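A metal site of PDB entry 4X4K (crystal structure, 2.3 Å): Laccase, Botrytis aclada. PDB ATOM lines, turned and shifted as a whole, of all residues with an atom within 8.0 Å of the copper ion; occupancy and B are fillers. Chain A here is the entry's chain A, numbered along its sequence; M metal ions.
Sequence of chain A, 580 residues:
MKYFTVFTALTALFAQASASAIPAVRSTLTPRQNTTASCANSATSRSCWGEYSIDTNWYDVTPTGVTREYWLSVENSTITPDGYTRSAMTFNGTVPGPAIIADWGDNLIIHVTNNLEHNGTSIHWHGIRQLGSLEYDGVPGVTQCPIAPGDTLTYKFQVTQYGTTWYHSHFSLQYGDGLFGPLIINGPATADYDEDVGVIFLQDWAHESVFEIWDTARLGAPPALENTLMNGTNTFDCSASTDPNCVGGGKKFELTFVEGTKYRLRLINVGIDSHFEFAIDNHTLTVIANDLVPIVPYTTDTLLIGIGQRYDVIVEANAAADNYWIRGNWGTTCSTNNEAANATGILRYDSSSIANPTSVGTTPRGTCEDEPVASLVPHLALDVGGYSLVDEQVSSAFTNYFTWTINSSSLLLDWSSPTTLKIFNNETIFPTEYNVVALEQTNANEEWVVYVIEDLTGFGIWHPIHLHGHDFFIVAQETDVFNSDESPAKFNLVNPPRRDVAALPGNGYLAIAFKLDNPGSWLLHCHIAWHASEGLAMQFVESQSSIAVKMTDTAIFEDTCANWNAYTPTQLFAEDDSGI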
ATOM      1  N   ASP A 273     -12.926 -22.150 -22.242  1.00  0.00           N
ATOM      2  CA  ASP A 273     -13.313 -21.384 -21.069  1.00  0.00           C
ATOM      3  C   ASP A 273     -14.806 -21.577 -20.853  1.00  0.00           C
ATOM      4  O   ASP A 273     -15.615 -20.741 -21.266  1.00  0.00           O
ATOM      5  CB  ASP A 273     -13.014 -19.899 -21.313  1.00  0.00           C
ATOM      6  CG  ASP A 273     -13.092 -19.070 -20.038  1.00  0.00           C
ATOM      7  OD1 ASP A 273     -13.432 -19.631 -18.970  1.00  0.00           O
ATOM      8  OD2 ASP A 273     -12.796 -17.867 -20.074  1.00  0.00           O
ATOM      9  N   ILE A 307     -13.292 -27.407 -16.299  1.00  0.00           N
ATOM     10  CA  ILE A 307     -12.572 -27.794 -17.517  1.00  0.00           C
ATOM     11  C   ILE A 307     -11.526 -28.829 -17.168  1.00  0.00           C
ATOM     12  O   ILE A 307     -10.748 -28.618 -16.242  1.00  0.00           O
ATOM     13  CB  ILE A 307     -11.862 -26.618 -18.233  1.00  0.00           C
ATOM     14  CG1 ILE A 307     -12.861 -25.575 -18.689  1.00  0.00           C
ATOM     15  CG2 ILE A 307     -11.077 -27.145 -19.439  1.00  0.00           C
ATOM     16  CD1 ILE A 307     -12.178 -24.380 -19.329  1.00  0.00           C
ATOM     17  N   VAL A 394      -2.198 -16.360  -6.446  1.00  0.00           N
ATOM     18  CA  VAL A 394      -2.510 -15.998  -7.806  1.00  0.00           C
ATOM     19  C   VAL A 394      -2.915 -14.526  -7.796  1.00  0.00           C
ATOM     20  O   VAL A 394      -3.769 -14.125  -7.008  1.00  0.00           O
ATOM     21  CB  VAL A 394      -3.605 -16.885  -8.459  1.00  0.00           C
ATOM     22  CG1 VAL A 394      -3.743 -16.535  -9.933  1.00  0.00           C
ATOM     23  CG2 VAL A 394      -3.272 -18.372  -8.347  1.00  0.00           C
ATOM     24  N   TRP A 404      -1.463 -13.713 -15.641  1.00  0.00           N
ATOM     25  CA  TRP A 404      -1.653 -14.129 -14.257  1.00  0.00           C
ATOM     26  C   TRP A 404      -0.286 -14.422 -13.660  1.00  0.00           C
ATOM     27  O   TRP A 404       0.613 -14.881 -14.359  1.00  0.00           O
ATOM     28  CB  TRP A 404      -2.495 -15.410 -14.186  1.00  0.00           C
ATOM     29  CG  TRP A 404      -3.756 -15.296 -14.950  1.00  0.00           C
ATOM     30  CD1 TRP A 404      -3.940 -15.577 -16.254  1.00  0.00           C
ATOM     31  CD2 TRP A 404      -4.994 -14.810 -14.445  1.00  0.00           C
ATOM     32  NE1 TRP A 404      -5.246 -15.313 -16.612  1.00  0.00           N
ATOM     33  CE2 TRP A 404      -5.915 -14.845 -15.519  1.00  0.00           C
ATOM     34  CE3 TRP A 404      -5.430 -14.355 -13.192  1.00  0.00           C
ATOM     35  CZ2 TRP A 404      -7.246 -14.452 -15.380  1.00  0.00           C
ATOM     36  CZ3 TRP A 404      -6.765 -13.975 -13.054  1.00  0.00           C
ATOM     37  CH2 TRP A 404      -7.646 -14.015 -14.134  1.00  0.00           C
ATOM     38  N   ILE A 461     -13.130 -15.690 -10.127  1.00  0.00           N
ATOM     39  CA  ILE A 461     -13.262 -16.795 -11.073  1.00  0.00           C
ATOM     40  C   ILE A 461     -12.889 -18.077 -10.360  1.00  0.00           C
ATOM     41  O   ILE A 461     -11.941 -18.111  -9.590  1.00  0.00           O
ATOM     42  CB  ILE A 461     -12.383 -16.647 -12.344  1.00  0.00           C
ATOM     43  CG1 ILE A 461     -12.728 -15.348 -13.109  1.00  0.00           C
ATOM     44  CG2 ILE A 461     -12.623 -17.846 -13.266  1.00  0.00           C
ATOM     45  CD1 ILE A 461     -11.613 -14.778 -13.978  1.00  0.00           C
ATOM     46  N   TRP A 462     -13.675 -19.130 -10.600  1.00  0.00           N
ATOM     47  CA  TRP A 462     -13.359 -20.466 -10.128  1.00  0.00           C
ATOM     48  C   TRP A 462     -12.423 -21.155 -11.123  1.00  0.00           C
ATOM     49  O   TRP A 462     -12.861 -21.654 -12.162  1.00  0.00           O
ATOM     50  CB  TRP A 462     -14.644 -21.254  -9.948  1.00  0.00           C
ATOM     51  CG  TRP A 462     -15.421 -20.756  -8.769  1.00  0.00           C
ATOM     52  CD1 TRP A 462     -15.986 -19.532  -8.632  1.00  0.00           C
ATOM     53  CD2 TRP A 462     -15.687 -21.464  -7.545  1.00  0.00           C
ATOM     54  NE1 TRP A 462     -16.599 -19.433  -7.412  1.00  0.00           N
ATOM     55  CE2 TRP A 462     -16.426 -20.597  -6.724  1.00  0.00           C
ATOM     56  CE3 TRP A 462     -15.376 -22.739  -7.077  1.00  0.00           C
ATOM     57  CZ2 TRP A 462     -16.872 -20.967  -5.447  1.00  0.00           C
ATOM     58  CZ3 TRP A 462     -15.816 -23.111  -5.792  1.00  0.00           C
ATOM     59  CH2 TRP A 462     -16.556 -22.226  -5.002  1.00  0.00           C
ATOM     60  N   HIS A 463     -11.120 -21.161 -10.810  1.00  0.00           N
ATOM     61  CA  HIS A 463     -10.139 -21.697 -11.741  1.00  0.00           C
ATOM     62  C   HIS A 463      -9.990 -23.210 -11.583  1.00  0.00           C
ATOM     63  O   HIS A 463      -9.717 -23.683 -10.480  1.00  0.00           O
ATOM     64  CB  HIS A 463      -8.800 -21.028 -11.555  1.00  0.00           C
ATOM     65  CG  HIS A 463      -8.850 -19.539 -11.626  1.00  0.00           C
ATOM     66  ND1 HIS A 463      -8.540 -18.836 -12.769  1.00  0.00           N
ATOM     67  CD2 HIS A 463      -9.155 -18.620 -10.680  1.00  0.00           C
ATOM     68  CE1 HIS A 463      -8.654 -17.542 -12.526  1.00  0.00           C
ATOM     69  NE2 HIS A 463      -9.041 -17.385 -11.272  1.00  0.00           N
ATOM     70  N   PRO A 464     -10.186 -23.970 -12.682  1.00  0.00           N
ATOM     71  CA  PRO A 464     -10.011 -25.410 -12.633  1.00  0.00           C
ATOM     72  C   PRO A 464      -8.500 -25.693 -12.627  1.00  0.00           C
ATOM     73  O   PRO A 464      -7.837 -25.530 -13.652  1.00  0.00           O
ATOM     74  CB  PRO A 464     -10.644 -25.879 -13.941  1.00  0.00           C
ATOM     75  CG  PRO A 464     -10.441 -24.737 -14.902  1.00  0.00           C
ATOM     76  CD  PRO A 464     -10.380 -23.481 -14.075  1.00  0.00           C
ATOM     77  N   ILE A 465      -7.976 -26.071 -11.472  1.00  0.00           N
ATOM     78  CA  ILE A 465      -6.562 -26.247 -11.276  1.00  0.00           C
ATOM     79  C   ILE A 465      -6.196 -27.696 -11.542  1.00  0.00           C
ATOM     80  O   ILE A 465      -6.724 -28.620 -10.904  1.00  0.00           O
ATOM     81  CB  ILE A 465      -6.122 -25.804  -9.865  1.00  0.00           C
ATOM     82  CG1 ILE A 465      -6.392 -24.291  -9.686  1.00  0.00           C
ATOM     83  CG2 ILE A 465      -4.651 -26.126  -9.653  1.00  0.00           C
ATOM     84  CD1 ILE A 465      -5.617 -23.373 -10.627  1.00  0.00           C
ATOM     85  N   LEU A 504      -9.999 -23.908  -7.889  1.00  0.00           N
ATOM     86  CA  LEU A 504      -9.564 -22.880  -6.942  1.00  0.00           C
ATOM     87  C   LEU A 504     -10.763 -21.921  -6.864  1.00  0.00           C
ATOM     88  O   LEU A 504     -11.087 -21.261  -7.862  1.00  0.00           O
ATOM     89  CB  LEU A 504      -8.318 -22.152  -7.466  1.00  0.00           C
ATOM     90  CG  LEU A 504      -8.061 -20.707  -7.062  1.00  0.00           C
ATOM     91  CD1 LEU A 504      -7.875 -20.614  -5.538  1.00  0.00           C
ATOM     92  CD2 LEU A 504      -6.815 -20.168  -7.768  1.00  0.00           C
ATOM     93  N   HIS A 525      -1.499 -25.958 -13.358  1.00  0.00           N
ATOM     94  CA  HIS A 525      -1.969 -24.807 -14.079  1.00  0.00           C
ATOM     95  C   HIS A 525      -3.468 -24.694 -14.057  1.00  0.00           C
ATOM     96  O   HIS A 525      -4.193 -25.677 -13.789  1.00  0.00           O
ATOM     97  CB  HIS A 525      -1.452 -24.836 -15.526  1.00  0.00           C
ATOM     98  CG  HIS A 525      -1.950 -26.004 -16.319  1.00  0.00           C
ATOM     99  ND1 HIS A 525      -3.047 -25.916 -17.157  1.00  0.00           N
ATOM    100  CD2 HIS A 525      -1.535 -27.290 -16.369  1.00  0.00           C
ATOM    101  CE1 HIS A 525      -3.271 -27.109 -17.698  1.00  0.00           C
ATOM    102  NE2 HIS A 525      -2.370 -27.949 -17.238  1.00  0.00           N
ATOM    103  N   CYS A 526      -3.955 -23.480 -14.331  1.00  0.00           N
ATOM    104  CA  CYS A 526      -5.357 -23.334 -14.595  1.00  0.00           C
ATOM    105  C   CYS A 526      -5.600 -24.001 -15.948  1.00  0.00           C
ATOM    106  O   CYS A 526      -4.797 -23.808 -16.887  1.00  0.00           O
ATOM    107  CB  CYS A 526      -5.769 -21.877 -14.647  1.00  0.00           C
ATOM    108  SG  CYS A 526      -7.537 -21.712 -14.961  1.00  0.00           S
ATOM    109  N   HIS A 527      -6.676 -24.786 -16.028  1.00  0.00           N
ATOM    110  CA  HIS A 527      -7.036 -25.453 -17.273  1.00  0.00           C
ATOM    111  C   HIS A 527      -7.905 -24.627 -18.214  1.00  0.00           C
ATOM    112  O   HIS A 527      -8.281 -25.098 -19.300  1.00  0.00           O
ATOM    113  CB  HIS A 527      -7.668 -26.823 -17.011  1.00  0.00           C
ATOM    114  CG  HIS A 527      -7.239 -27.877 -17.998  1.00  0.00           C
ATOM    115  ND1 HIS A 527      -7.439 -27.753 -19.357  1.00  0.00           N
ATOM    116  CD2 HIS A 527      -6.622 -29.074 -17.810  1.00  0.00           C
ATOM    117  CE1 HIS A 527      -6.957 -28.820 -19.969  1.00  0.00           C
ATOM    118  NE2 HIS A 527      -6.472 -29.646 -19.059  1.00  0.00           N
ATOM    119  N   ILE A 528      -8.238 -23.392 -17.809  1.00  0.00           N
ATOM    120  CA  ILE A 528      -8.902 -22.463 -18.724  1.00  0.00           C
ATOM    121  C   ILE A 528      -7.846 -22.055 -19.753  1.00  0.00           C
ATOM    122  O   ILE A 528      -6.777 -21.534 -19.393  1.00  0.00           O
ATOM    123  CB  ILE A 528      -9.468 -21.234 -18.005  1.00  0.00           C
ATOM    124  CG1 ILE A 528     -10.667 -21.627 -17.162  1.00  0.00           C
ATOM    125  CG2 ILE A 528      -9.953 -20.244 -19.029  1.00  0.00           C
ATOM    126  CD1 ILE A 528     -11.093 -20.569 -16.138  1.00  0.00           C
ATOM    127  N   ALA A 529      -8.120 -22.301 -21.033  1.00  0.00           N
ATOM    128  CA  ALA A 529      -7.032 -22.236 -21.997  1.00  0.00           C
ATOM    129  C   ALA A 529      -6.390 -20.849 -22.008  1.00  0.00           C
ATOM    130  O   ALA A 529      -5.163 -20.745 -22.063  1.00  0.00           O
ATOM    131  CB  ALA A 529      -7.512 -22.638 -23.380  1.00  0.00           C
ATOM    132  N   TRP A 530      -7.203 -19.799 -21.950  1.00  0.00           N
ATOM    133  CA  TRP A 530      -6.677 -18.451 -21.930  1.00  0.00           C
ATOM    134  C   TRP A 530      -5.771 -18.235 -20.715  1.00  0.00           C
ATOM    135  O   TRP A 530      -4.734 -17.590 -20.800  1.00  0.00           O
ATOM    136  CB  TRP A 530      -7.793 -17.396 -21.920  1.00  0.00           C
ATOM    137  CG  TRP A 530      -8.859 -17.564 -22.970  1.00  0.00           C
ATOM    138  CD1 TRP A 530     -10.186 -17.788 -22.755  1.00  0.00           C
ATOM    139  CD2 TRP A 530      -8.696 -17.508 -24.405  1.00  0.00           C
ATOM    140  NE1 TRP A 530     -10.862 -17.879 -23.943  1.00  0.00           N
ATOM    141  CE2 TRP A 530      -9.965 -17.703 -24.979  1.00  0.00           C
ATOM    142  CE3 TRP A 530      -7.603 -17.311 -25.258  1.00  0.00           C
ATOM    143  CZ2 TRP A 530     -10.173 -17.694 -26.355  1.00  0.00           C
ATOM    144  CZ3 TRP A 530      -7.814 -17.310 -26.622  1.00  0.00           C
ATOM    145  CH2 TRP A 530      -9.080 -17.501 -27.159  1.00  0.00           C
ATOM    146  N   HIS A 531      -6.132 -18.832 -19.579  1.00  0.00           N
ATOM    147  CA  HIS A 531      -5.372 -18.561 -18.370  1.00  0.00           C
ATOM    148  C   HIS A 531      -4.019 -19.201 -18.385  1.00  0.00           C
ATOM    149  O   HIS A 531      -3.045 -18.588 -17.931  1.00  0.00           O
ATOM    150  CB  HIS A 531      -6.175 -18.974 -17.157  1.00  0.00           C
ATOM    151  CG  HIS A 531      -7.396 -18.149 -16.992  1.00  0.00           C
ATOM    152  ND1 HIS A 531      -8.224 -18.233 -15.901  1.00  0.00           N
ATOM    153  CD2 HIS A 531      -7.919 -17.192 -17.796  1.00  0.00           C
ATOM    154  CE1 HIS A 531      -9.230 -17.380 -16.056  1.00  0.00           C
ATOM    155  NE2 HIS A 531      -9.051 -16.726 -17.184  1.00  0.00           N
ATOM    156  N   ALA A 532      -3.981 -20.412 -18.927  1.00  0.00           N
ATOM    157  CA  ALA A 532      -2.777 -21.196 -19.069  1.00  0.00           C
ATOM    158  C   ALA A 532      -1.816 -20.424 -19.970  1.00  0.00           C
ATOM    159  O   ALA A 532      -0.678 -20.179 -19.592  1.00  0.00           O
ATOM    160  CB  ALA A 532      -3.115 -22.549 -19.666  1.00  0.00           C
ATOM    161  N   GLU A 534      -1.943 -17.400 -20.523  1.00  0.00           N
ATOM    162  CA  GLU A 534      -1.590 -16.188 -19.777  1.00  0.00           C
ATOM    163  C   GLU A 534      -0.696 -16.462 -18.550  1.00  0.00           C
ATOM    164  O   GLU A 534      -0.614 -15.622 -17.624  1.00  0.00           O
ATOM    165  CB  GLU A 534      -2.832 -15.378 -19.412  1.00  0.00           C
ATOM    166  CG  GLU A 534      -3.428 -14.651 -20.626  1.00  0.00           C
ATOM    167  CD  GLU A 534      -4.946 -14.525 -20.598  1.00  0.00           C
ATOM    168  OE1 GLU A 534      -5.567 -14.661 -19.506  1.00  0.00           O
ATOM    169  OE2 GLU A 534      -5.539 -14.291 -21.698  1.00  0.00           O
ATOM    170  N   LEU A 536      -0.830 -18.622 -15.939  1.00  0.00           N
ATOM    171  CA  LEU A 536      -1.402 -19.100 -14.668  1.00  0.00           C
ATOM    172  C   LEU A 536      -0.987 -20.536 -14.398  1.00  0.00           C
ATOM    173  O   LEU A 536      -1.759 -21.518 -14.563  1.00  0.00           O
ATOM    174  CB  LEU A 536      -2.948 -18.967 -14.607  1.00  0.00           C
ATOM    175  CG  LEU A 536      -3.456 -18.701 -13.184  1.00  0.00           C
ATOM    176  CD1 LEU A 536      -4.939 -18.333 -13.147  1.00  0.00           C
ATOM    177  CD2 LEU A 536      -3.225 -19.850 -12.230  1.00  0.00           C
HETATM  178 CU    CU M   1      -8.032 -19.631 -14.502  1.00  0.00          CU
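The backbone carbonyl oxygen of Leu 536 is in hydrogen-bond range of the backbone NH of Cys 526 (3.0 Å). The backbone carbonyl oxygen (O) of His 531 lies within hydrogen-bond range of the backbone NH (N) of Leu 536 (3.0 Å). O of His 463 lies within hydrogen-bond range of N of Leu 504, at 2.6 Å. A ring nitrogen (NE2) of His 463 sits close to the backbone carbonyl oxygen of Ile 461 (3.4 Å). The side-chain sulfur of Cys 526 sits close to the backbone NH of Ile 528.
Ile 528 touches the copper ion. Leu 536 touches the copper ion (CD1 to CU, 3.6 Å). Within 4 Å of the copper ion: His 463, Cys 526, Ile 528, His 531 and Leu 536. The nearest printed residue that does not touch the copper ion is Pro 464 (4.5 Å).
The copper ion is bound by a ring nitrogen (ND1) of His 463, a ring nitrogen (ND1) of His 531 and the side-chain sulfur (SG) of Cys 526.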
